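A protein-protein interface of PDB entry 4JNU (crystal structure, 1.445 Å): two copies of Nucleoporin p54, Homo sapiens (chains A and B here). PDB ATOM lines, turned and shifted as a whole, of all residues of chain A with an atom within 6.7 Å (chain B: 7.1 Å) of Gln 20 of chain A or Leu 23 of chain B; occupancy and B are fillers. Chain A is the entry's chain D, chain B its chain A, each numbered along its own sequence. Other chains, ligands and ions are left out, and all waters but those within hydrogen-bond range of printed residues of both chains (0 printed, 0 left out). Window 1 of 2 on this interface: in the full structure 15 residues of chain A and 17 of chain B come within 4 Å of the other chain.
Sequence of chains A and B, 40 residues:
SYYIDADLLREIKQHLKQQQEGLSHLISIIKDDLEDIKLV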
ATOM      1  N   HIS A  15      13.997   6.475 -28.943  1.00  0.00           N
ATOM      2  CA  HIS A  15      13.642   5.045 -28.940  1.00  0.00           C
ATOM      3  C   HIS A  15      13.732   4.447 -27.547  1.00  0.00           C
ATOM      4  O   HIS A  15      12.861   3.642 -27.157  1.00  0.00           O
ATOM      5  CB  HIS A  15      14.545   4.248 -29.867  1.00  0.00           C
ATOM      6  CG  HIS A  15      14.162   4.325 -31.311  1.00  0.00           C
ATOM      7  ND1 HIS A  15      13.035   3.720 -31.824  1.00  0.00           N
ATOM      8  CD2 HIS A  15      14.786   4.910 -32.362  1.00  0.00           C
ATOM      9  CE1 HIS A  15      12.970   3.945 -33.125  1.00  0.00           C
ATOM     10  NE2 HIS A  15      14.021   4.662 -33.475  1.00  0.00           N
ATOM     11  N   LEU A  16      14.762   4.809 -26.799  1.00  0.00           N
ATOM     12  CA  LEU A  16      14.902   4.324 -25.421  1.00  0.00           C
ATOM     13  C   LEU A  16      13.798   4.822 -24.510  1.00  0.00           C
ATOM     14  O   LEU A  16      13.339   4.077 -23.652  1.00  0.00           O
ATOM     15  CB  LEU A  16      16.268   4.689 -24.849  1.00  0.00           C
ATOM     16  CG  LEU A  16      17.440   3.991 -25.526  1.00  0.00           C
ATOM     17  CD1 LEU A  16      18.736   4.644 -25.074  1.00  0.00           C
ATOM     18  CD2 LEU A  16      17.433   2.518 -25.207  1.00  0.00           C
ATOM     19  N   LYS A  17      13.367   6.066 -24.689  1.00  0.00           N
ATOM     20  CA  LYS A  17      12.232   6.585 -23.929  1.00  0.00           C
ATOM     21  C   LYS A  17      10.959   5.811 -24.274  1.00  0.00           C
ATOM     22  O   LYS A  17      10.137   5.542 -23.401  1.00  0.00           O
ATOM     23  CB  LYS A  17      12.025   8.067 -24.215  1.00  0.00           C
ATOM     24  CG  LYS A  17      13.112   8.969 -23.692  1.00  0.00           C
ATOM     25  CD  LYS A  17      12.794  10.393 -24.104  1.00  0.00           C
ATOM     26  CE  LYS A  17      13.652  11.396 -23.413  1.00  0.00           C
ATOM     27  NZ  LYS A  17      13.151  12.750 -23.769  1.00  0.00           N
ATOM     28  N   GLN A  18      10.778   5.461 -25.544  1.00  0.00           N
ATOM     29  CA  GLN A  18       9.610   4.695 -25.955  1.00  0.00           C
ATOM     30  C   GLN A  18       9.652   3.305 -25.325  1.00  0.00           C
ATOM     31  O   GLN A  18       8.637   2.786 -24.848  1.00  0.00           O
ATOM     32  CB  GLN A  18       9.543   4.598 -27.476  1.00  0.00           C
ATOM     33  CG  GLN A  18       9.083   5.879 -28.146  1.00  0.00           C
ATOM     34  CD  GLN A  18       8.786   5.727 -29.631  1.00  0.00           C
ATOM     35  OE1 GLN A  18       9.015   6.654 -30.410  1.00  0.00           O
ATOM     36  NE2 GLN A  18       8.248   4.576 -30.027  1.00  0.00           N
ATOM     37  N   GLN A  19      10.839   2.721 -25.275  1.00  0.00           N
ATOM     38  CA  GLN A  19      10.992   1.403 -24.668  1.00  0.00           C
ATOM     39  C   GLN A  19      10.770   1.456 -23.165  1.00  0.00           C
ATOM     40  O   GLN A  19      10.186   0.529 -22.578  1.00  0.00           O
ATOM     41  CB  GLN A  19      12.346   0.793 -25.014  1.00  0.00           C
ATOM     42  CG  GLN A  19      12.388   0.372 -26.471  1.00  0.00           C
ATOM     43  CD  GLN A  19      13.443  -0.647 -26.800  1.00  0.00           C
ATOM     44  OE1 GLN A  19      14.173  -0.491 -27.789  1.00  0.00           O
ATOM     45  NE2 GLN A  19      13.524  -1.706 -26.009  1.00  0.00           N
ATOM     46  N   GLN A  20      11.223   2.538 -22.545  1.00  0.00           N
ATOM     47  CA  GLN A  20      11.007   2.756 -21.125  1.00  0.00           C
ATOM     48  C   GLN A  20       9.522   2.851 -20.826  1.00  0.00           C
ATOM     49  O   GLN A  20       9.054   2.296 -19.830  1.00  0.00           O
ATOM     50  CB  GLN A  20      11.719   4.031 -20.684  1.00  0.00           C
ATOM     51  CG  GLN A  20      11.684   4.269 -19.191  1.00  0.00           C
ATOM     52  CD  GLN A  20      12.595   3.326 -18.436  1.00  0.00           C
ATOM     53  OE1 GLN A  20      12.420   2.103 -18.474  1.00  0.00           O
ATOM     54  NE2 GLN A  20      13.589   3.886 -17.757  1.00  0.00           N
ATOM     55  N   GLU A  21       8.767   3.528 -21.691  1.00  0.00           N
ATOM     56  CA  GLU A  21       7.309   3.592 -21.536  1.00  0.00           C
ATOM     57  C   GLU A  21       6.661   2.216 -21.684  1.00  0.00           C
ATOM     58  O   GLU A  21       5.711   1.905 -20.983  1.00  0.00           O
ATOM     59  CB  GLU A  21       6.695   4.576 -22.533  1.00  0.00           C
ATOM     60  CG  GLU A  21       5.189   4.756 -22.376  1.00  0.00           C
ATOM     61  CD  GLU A  21       4.757   4.997 -20.933  1.00  0.00           C
ATOM     62  OE1 GLU A  21       5.403   5.816 -20.239  1.00  0.00           O
ATOM     63  OE2 GLU A  21       3.766   4.366 -20.494  1.00  0.00           O
ATOM     64  N   GLY A  22       7.180   1.404 -22.595  1.00  0.00           N
ATOM     65  CA  GLY A  22       6.742   0.026 -22.729  1.00  0.00           C
ATOM     66  C   GLY A  22       6.969  -0.780 -21.461  1.00  0.00           C
ATOM     67  O   GLY A  22       6.105  -1.537 -21.054  1.00  0.00           O
ATOM     68  N   LEU A  23       8.137  -0.651 -20.839  1.00  0.00           N
ATOM     69  CA  LEU A  23       8.371  -1.355 -19.590  1.00  0.00           C
ATOM     70  C   LEU A  23       7.428  -0.848 -18.502  1.00  0.00           C
ATOM     71  O   LEU A  23       6.920  -1.631 -17.714  1.00  0.00           O
ATOM     72  CB  LEU A  23       9.816  -1.242 -19.123  1.00  0.00           C
ATOM     73  CG  LEU A  23      10.861  -1.915 -19.993  1.00  0.00           C
ATOM     74  CD1 LEU A  23      12.281  -1.674 -19.430  1.00  0.00           C
ATOM     75  CD2 LEU A  23      10.558  -3.410 -20.151  1.00  0.00           C
ATOM     76  N   SER A  24       7.199   0.463 -18.458  1.00  0.00           N
ATOM     77  CA  SER A  24       6.273   1.031 -17.484  1.00  0.00           C
ATOM     78  C   SER A  24       4.898   0.430 -17.668  1.00  0.00           C
ATOM     79  O   SER A  24       4.223   0.109 -16.694  1.00  0.00           O
ATOM     80  CB  SER A  24       6.183   2.558 -17.598  1.00  0.00           C
ATOM     81  OG  SER A  24       7.365   3.175 -17.132  1.00  0.00           O
ATOM     82  N   HIS A  25       4.478   0.308 -18.922  1.00  0.00           N
ATOM     83  CA  HIS A  25       3.169  -0.257 -19.230  1.00  0.00           C
ATOM     84  C   HIS A  25       3.069  -1.707 -18.762  1.00  0.00           C
ATOM     85  O   HIS A  25       2.044  -2.116 -18.211  1.00  0.00           O
ATOM     86  CB  HIS A  25       2.887  -0.143 -20.726  1.00  0.00           C
ATOM     87  CG  HIS A  25       1.630  -0.826 -21.154  1.00  0.00           C
ATOM     88  ND1 HIS A  25       0.377  -0.310 -20.896  1.00  0.00           N
ATOM     89  CD2 HIS A  25       1.431  -1.990 -21.814  1.00  0.00           C
ATOM     90  CE1 HIS A  25      -0.539  -1.126 -21.384  1.00  0.00           C
ATOM     91  NE2 HIS A  25       0.073  -2.153 -21.946  1.00  0.00           N
ATOM     92  N   ILE A  27       4.901  -3.093 -16.322  1.00  0.00           N
ATOM     93  CA  ILE A  27       4.881  -3.026 -14.867  1.00  0.00           C
ATOM     94  C   ILE A  27       3.482  -2.655 -14.387  1.00  0.00           C
ATOM     95  O   ILE A  27       2.981  -3.215 -13.409  1.00  0.00           O
ATOM     96  CB  ILE A  27       5.960  -2.055 -14.343  1.00  0.00           C
ATOM     97  CG1 ILE A  27       7.344  -2.654 -14.620  1.00  0.00           C
ATOM     98  CG2 ILE A  27       5.804  -1.794 -12.856  1.00  0.00           C
ATOM     99  CD1 ILE A  27       8.511  -1.668 -14.504  1.00  0.00           C
ATOM    100  N   LEU B  16      11.939  -6.603 -14.271  1.00  0.00           N
ATOM    101  CA  LEU B  16      11.529  -5.476 -15.108  1.00  0.00           C
ATOM    102  C   LEU B  16      12.024  -4.160 -14.508  1.00  0.00           C
ATOM    103  O   LEU B  16      12.412  -3.265 -15.231  1.00  0.00           O
ATOM    104  CB  LEU B  16      10.009  -5.454 -15.288  1.00  0.00           C
ATOM    105  CG  LEU B  16       9.464  -6.592 -16.163  1.00  0.00           C
ATOM    106  CD1 LEU B  16       7.946  -6.581 -16.096  1.00  0.00           C
ATOM    107  CD2 LEU B  16       9.923  -6.531 -17.615  1.00  0.00           C
ATOM    108  N   LYS B  17      12.029  -4.077 -13.187  1.00  0.00           N
ATOM    109  CA  LYS B  17      12.559  -2.899 -12.525  1.00  0.00           C
ATOM    110  C   LYS B  17      14.055  -2.738 -12.783  1.00  0.00           C
ATOM    111  O   LYS B  17      14.552  -1.620 -12.935  1.00  0.00           O
ATOM    112  CB  LYS B  17      12.245  -2.953 -11.037  1.00  0.00           C
ATOM    113  CG  LYS B  17      10.779  -2.664 -10.773  1.00  0.00           C
ATOM    114  CD  LYS B  17      10.473  -2.492  -9.300  1.00  0.00           C
ATOM    115  CE  LYS B  17       9.443  -1.389  -9.063  1.00  0.00           C
ATOM    116  NZ  LYS B  17       8.721  -0.917 -10.284  1.00  0.00           N
ATOM    117  N   GLN B  18      14.777  -3.848 -12.851  1.00  0.00           N
ATOM    118  CA  GLN B  18      16.199  -3.818 -13.187  1.00  0.00           C
ATOM    119  C   GLN B  18      16.408  -3.381 -14.646  1.00  0.00           C
ATOM    120  O   GLN B  18      17.324  -2.593 -14.951  1.00  0.00           O
ATOM    121  CB  GLN B  18      16.841  -5.190 -12.918  1.00  0.00           C
ATOM    122  CG  GLN B  18      16.928  -5.524 -11.429  1.00  0.00           C
ATOM    123  CD  GLN B  18      17.749  -4.511 -10.653  1.00  0.00           C
ATOM    124  OE1 GLN B  18      17.237  -3.846  -9.750  1.00  0.00           O
ATOM    125  NE2 GLN B  18      19.023  -4.380 -11.005  1.00  0.00           N
ATOM    126  N   GLN B  19      15.556  -3.844 -15.556  1.00  0.00           N
ATOM    127  CA  GLN B  19      15.592  -3.381 -16.935  1.00  0.00           C
ATOM    128  C   GLN B  19      15.331  -1.871 -17.010  1.00  0.00           C
ATOM    129  O   GLN B  19      16.007  -1.151 -17.762  1.00  0.00           O
ATOM    130  CB  GLN B  19      14.573  -4.142 -17.795  1.00  0.00           C
ATOM    131  CG  GLN B  19      14.980  -5.557 -18.118  1.00  0.00           C
ATOM    132  CD  GLN B  19      15.881  -5.631 -19.325  1.00  0.00           C
ATOM    133  OE1 GLN B  19      15.491  -5.278 -20.438  1.00  0.00           O
ATOM    134  NE2 GLN B  19      17.098  -6.054 -19.106  1.00  0.00           N
ATOM    135  N   GLN B  20      14.353  -1.382 -16.251  1.00  0.00           N
ATOM    136  CA  GLN B  20      14.071   0.053 -16.251  1.00  0.00           C
ATOM    137  C   GLN B  20      15.273   0.849 -15.754  1.00  0.00           C
ATOM    138  O   GLN B  20      15.573   1.901 -16.304  1.00  0.00           O
ATOM    139  CB  GLN B  20      12.848   0.396 -15.408  1.00  0.00           C
ATOM    140  CG  GLN B  20      11.523   0.048 -16.093  1.00  0.00           C
ATOM    141  CD  GLN B  20      10.438   1.113 -15.896  1.00  0.00           C
ATOM    142  OE1 GLN B  20      10.023   1.792 -16.841  1.00  0.00           O
ATOM    143  NE2 GLN B  20       9.968   1.243 -14.672  1.00  0.00           N
ATOM    144  N   GLU B  21      15.959   0.352 -14.722  1.00  0.00           N
ATOM    145  CA  GLU B  21      17.181   1.001 -14.256  1.00  0.00           C
ATOM    146  C   GLU B  21      18.228   1.046 -15.362  1.00  0.00           C
ATOM    147  O   GLU B  21      18.892   2.073 -15.538  1.00  0.00           O
ATOM    148  CB  GLU B  21      17.745   0.326 -12.998  1.00  0.00           C
ATOM    149  CG  GLU B  21      16.885   0.520 -11.762  1.00  0.00           C
ATOM    150  CD  GLU B  21      17.416  -0.229 -10.552  1.00  0.00           C
ATOM    151  OE1 GLU B  21      18.465  -0.901 -10.662  1.00  0.00           O
ATOM    152  OE2 GLU B  21      16.797  -0.120  -9.470  1.00  0.00           O
ATOM    153  N   GLY B  22      18.365  -0.020 -16.126  1.00  0.00           N
ATOM    154  CA  GLY B  22      19.324  -0.020 -17.213  1.00  0.00           C
ATOM    155  C   GLY B  22      19.012   1.008 -18.272  1.00  0.00           C
ATOM    156  O   GLY B  22      19.926   1.694 -18.750  1.00  0.00           O
ATOM    157  N   LEU B  23      17.749   1.133 -18.659  1.00  0.00           N
ATOM    158  CA  LEU B  23      17.378   2.134 -19.657  1.00  0.00           C
ATOM    159  C   LEU B  23      17.560   3.546 -19.116  1.00  0.00           C
ATOM    160  O   LEU B  23      17.981   4.433 -19.853  1.00  0.00           O
ATOM    161  CB  LEU B  23      15.936   1.947 -20.124  1.00  0.00           C
ATOM    162  CG  LEU B  23      15.604   0.674 -20.912  1.00  0.00           C
ATOM    163  CD1 LEU B  23      14.188   0.809 -21.443  1.00  0.00           C
ATOM    164  CD2 LEU B  23      16.579   0.415 -22.057  1.00  0.00           C
ATOM    165  N   SER B  24      17.237   3.763 -17.843  1.00  0.00           N
ATOM    166  CA  SER B  24      17.446   5.071 -17.235  1.00  0.00           C
ATOM    167  C   SER B  24      18.919   5.451 -17.284  1.00  0.00           C
ATOM    168  O   SER B  24      19.273   6.572 -17.686  1.00  0.00           O
ATOM    169  CB  SER B  24      16.967   5.069 -15.792  1.00  0.00           C
ATOM    170  OG  SER B  24      15.556   4.964 -15.713  1.00  0.00           O
ATOM    171  N   HIS B  25      19.793   4.529 -16.891  1.00  0.00           N
ATOM    172  CA  HIS B  25      21.228   4.825 -16.902  1.00  0.00           C
ATOM    173  C   HIS B  25      21.704   5.175 -18.294  1.00  0.00           C
ATOM    174  O   HIS B  25      22.512   6.080 -18.462  1.00  0.00           O
ATOM    175  CB  HIS B  25      22.037   3.652 -16.357  1.00  0.00           C
ATOM    176  CG  HIS B  25      21.838   3.406 -14.900  1.00  0.00           C
ATOM    177  ND1 HIS B  25      21.498   4.401 -14.014  1.00  0.00           N
ATOM    178  CD2 HIS B  25      21.900   2.260 -14.177  1.00  0.00           C
ATOM    179  CE1 HIS B  25      21.377   3.886 -12.803  1.00  0.00           C
ATOM    180  NE2 HIS B  25      21.613   2.590 -12.874  1.00  0.00           N
ATOM    181  N   LEU B  26      21.196   4.492 -19.307  1.00  0.00           N
ATOM    182  CA  LEU B  26      21.639   4.734 -20.665  1.00  0.00           C
ATOM    183  C   LEU B  26      21.081   6.052 -21.196  1.00  0.00           C
ATOM    184  O   LEU B  26      21.777   6.793 -21.884  1.00  0.00           O
ATOM    185  CB  LEU B  26      21.260   3.574 -21.579  1.00  0.00           C
ATOM    186  CG  LEU B  26      21.831   3.705 -22.989  1.00  0.00           C
ATOM    187  CD1 LEU B  26      23.334   3.920 -22.966  1.00  0.00           C
ATOM    188  CD2 LEU B  26      21.496   2.452 -23.752  1.00  0.00           C
ATOM    189  N   ILE B  27      19.826   6.343 -20.895  1.00  0.00           N
ATOM    190  CA  ILE B  27      19.259   7.637 -21.248  1.00  0.00           C
ATOM    191  C   ILE B  27      20.081   8.759 -20.607  1.00  0.00           C
ATOM    192  O   ILE B  27      20.398   9.749 -21.274  1.00  0.00           O
ATOM    193  CB  ILE B  27      17.787   7.730 -20.858  1.00  0.00           C
ATOM    194  CG1 ILE B  27      16.960   6.808 -21.770  1.00  0.00           C
ATOM    195  CG2 ILE B  27      17.296   9.194 -20.939  1.00  0.00           C
ATOM    196  CD1 ILE B  27      15.558   6.542 -21.235  1.00  0.00           C
ATOM    197  N   SER B  28      20.460   8.595 -19.340  1.00  0.00           N
ATOM    198  CA  SER B  28      21.284   9.591 -18.661  1.00  0.00           C
ATOM    199  C   SER B  28      22.623   9.786 -19.369  1.00  0.00           C
ATOM    200  O   SER B  28      23.109  10.908 -19.502  1.00  0.00           O
ATOM    201  CB  SER B  28      21.520   9.171 -17.216  1.00  0.00           C
ATOM    202  OG  SER B  28      20.325   9.299 -16.469  1.00  0.00           O
ATOM    203  N   ILE B  29      23.239   8.695 -19.802  1.00  0.00           N
ATOM    204  CA  ILE B  29      24.520   8.768 -20.489  1.00  0.00           C
ATOM    205  C   ILE B  29      24.394   9.543 -21.782  1.00  0.00           C
ATOM    206  O   ILE B  29      25.226  10.390 -22.081  1.00  0.00           O
ATOM    207  CB  ILE B  29      25.059   7.355 -20.742  1.00  0.00           C
ATOM    208  CG1 ILE B  29      25.631   6.779 -19.450  1.00  0.00           C
ATOM    209  CG2 ILE B  29      26.146   7.360 -21.814  1.00  0.00           C
ATOM    210  CD1 ILE B  29      25.843   5.256 -19.518  1.00  0.00           C
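The side-chain amide oxygen (OE1) of Gln 20 of chain A sits close to the side-chain amide oxygen (OE1) of Gln 20 of chain B (2.9 Å).
OE1 of Gln 20 of chain B lies within hydrogen-bond range of OG of Ser 24 of chain A (3.0 Å).
The side-chain hydroxyl (OG) of Ser 24 of chain B lies within hydrogen-bond range of the side-chain amide nitrogen (NE2) of Gln 20 of chain A (3.0 Å).
Among the printed residues, pairs that only touch across the chains: Ile 27 of chain A with Gln 20 of chain B (3.3 Å), Gln 20 of chain A with Leu 23 of chain B (3.6 Å), Leu 23 of chain A with Gln 20 of chain B (3.7 Å), Leu 23 of chain A with Leu 23 of chain B (3.7 Å), Leu 23 of chain A with Gln 19 of chain B (3.7 Å), Leu 16 of chain A with Leu 26 of chain B (3.8 Å), Leu 16 of chain A with Ile 27 of chain B (3.8 Å), Gln 19 of chain A with Leu 23 of chain B (3.9 Å), Leu 16 of chain A with Leu 23 of chain B (3.9 Å), Ile 27 of chain A with Leu 16 of chain B (3.9 Å) and Ile 27 of chain A with Lys 17 of chain B (3.99 Å).
The backbone carbonyl oxygen of Gln 20 of chain B is in hydrogen-bond range of the side-chain hydroxyl of Ser 24 of chain B.
The side-chain hydroxyl (OG) of Ser 28 of chain B sits at hydrogen-bond distance from the backbone carbonyl oxygen (O) of Ser 24 of chain B, 3.2 Å away.
OG of Ser 24 of chain A lies within hydrogen-bond range of O of Gln 20 of chain A, at 3.3 Å.
Of the 12 printed residues of chain A, 6 touch a printed residue of chain B.
Printed residues of chain A that touch a printed residue of chain B: Leu 16, Gln 19, Gln 20, Leu 23, Ser 24 and Ile 27.
Hydrophobic or aromatic side chains of chain A within 4 Å of the printed part of chain B: Leu 16, Leu 23 and Ile 27.
Of the 14 printed residues of chain B, 8 touch a printed residue of chain A.
Hydrophobic or aromatic side chains of chain B that line the printed part of chain A: Leu 16, Leu 23, Leu 26 and Ile 27.
Among the printed residues, 14 pairs touch across the chains.
Leu 16 of chain A touches Leu 23 of chain B, but with the chains exchanged Leu 23 of chain A does not touch Leu 16 of chain B (4.1 Å).
Leu 16 of chain A touches Ile 27 of chain B, and with the chains exchanged Ile 27 of chain A touches Leu 16 of chain B.
Gln 20 of chain A touches Ser 24 of chain B, and with the chains exchanged Ser 24 of chain A touches Gln 20 of chain B.
Ile 27 of chain A touches Lys 17 of chain B, but with the chains exchanged Lys 17 of chain A does not touch Ile 27 of chain B (4.1 Å).
Positions printed for both chains: 16, 17, 18, 19, 20, 21, 22, 23, 24, 25 and 27.
Of the 14 pairs that touch across the chains among the printed residues, 10 have their exchanged pair printed and touching as well.
Of the printed residues of chain B, Gln 19 of chain A touches Leu 23 (3.9 Å).
Of the printed residues of chain B, Gln 20 of chain A touches Gln 20, Leu 23 and Ser 24.
Gln 18 of chain B touches none of the printed residues of chain A.
Of the printed residues of chain A, Gln 19 of chain B touches Leu 23.
The nearest printed residue of chain B that does not touch Gln 20 of chain A is Ile 27 of chain B (4.6 Å).
The nearest printed residue of chain B that does not touch Ser 24 of chain A is Leu 16 of chain B (7.2 Å).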
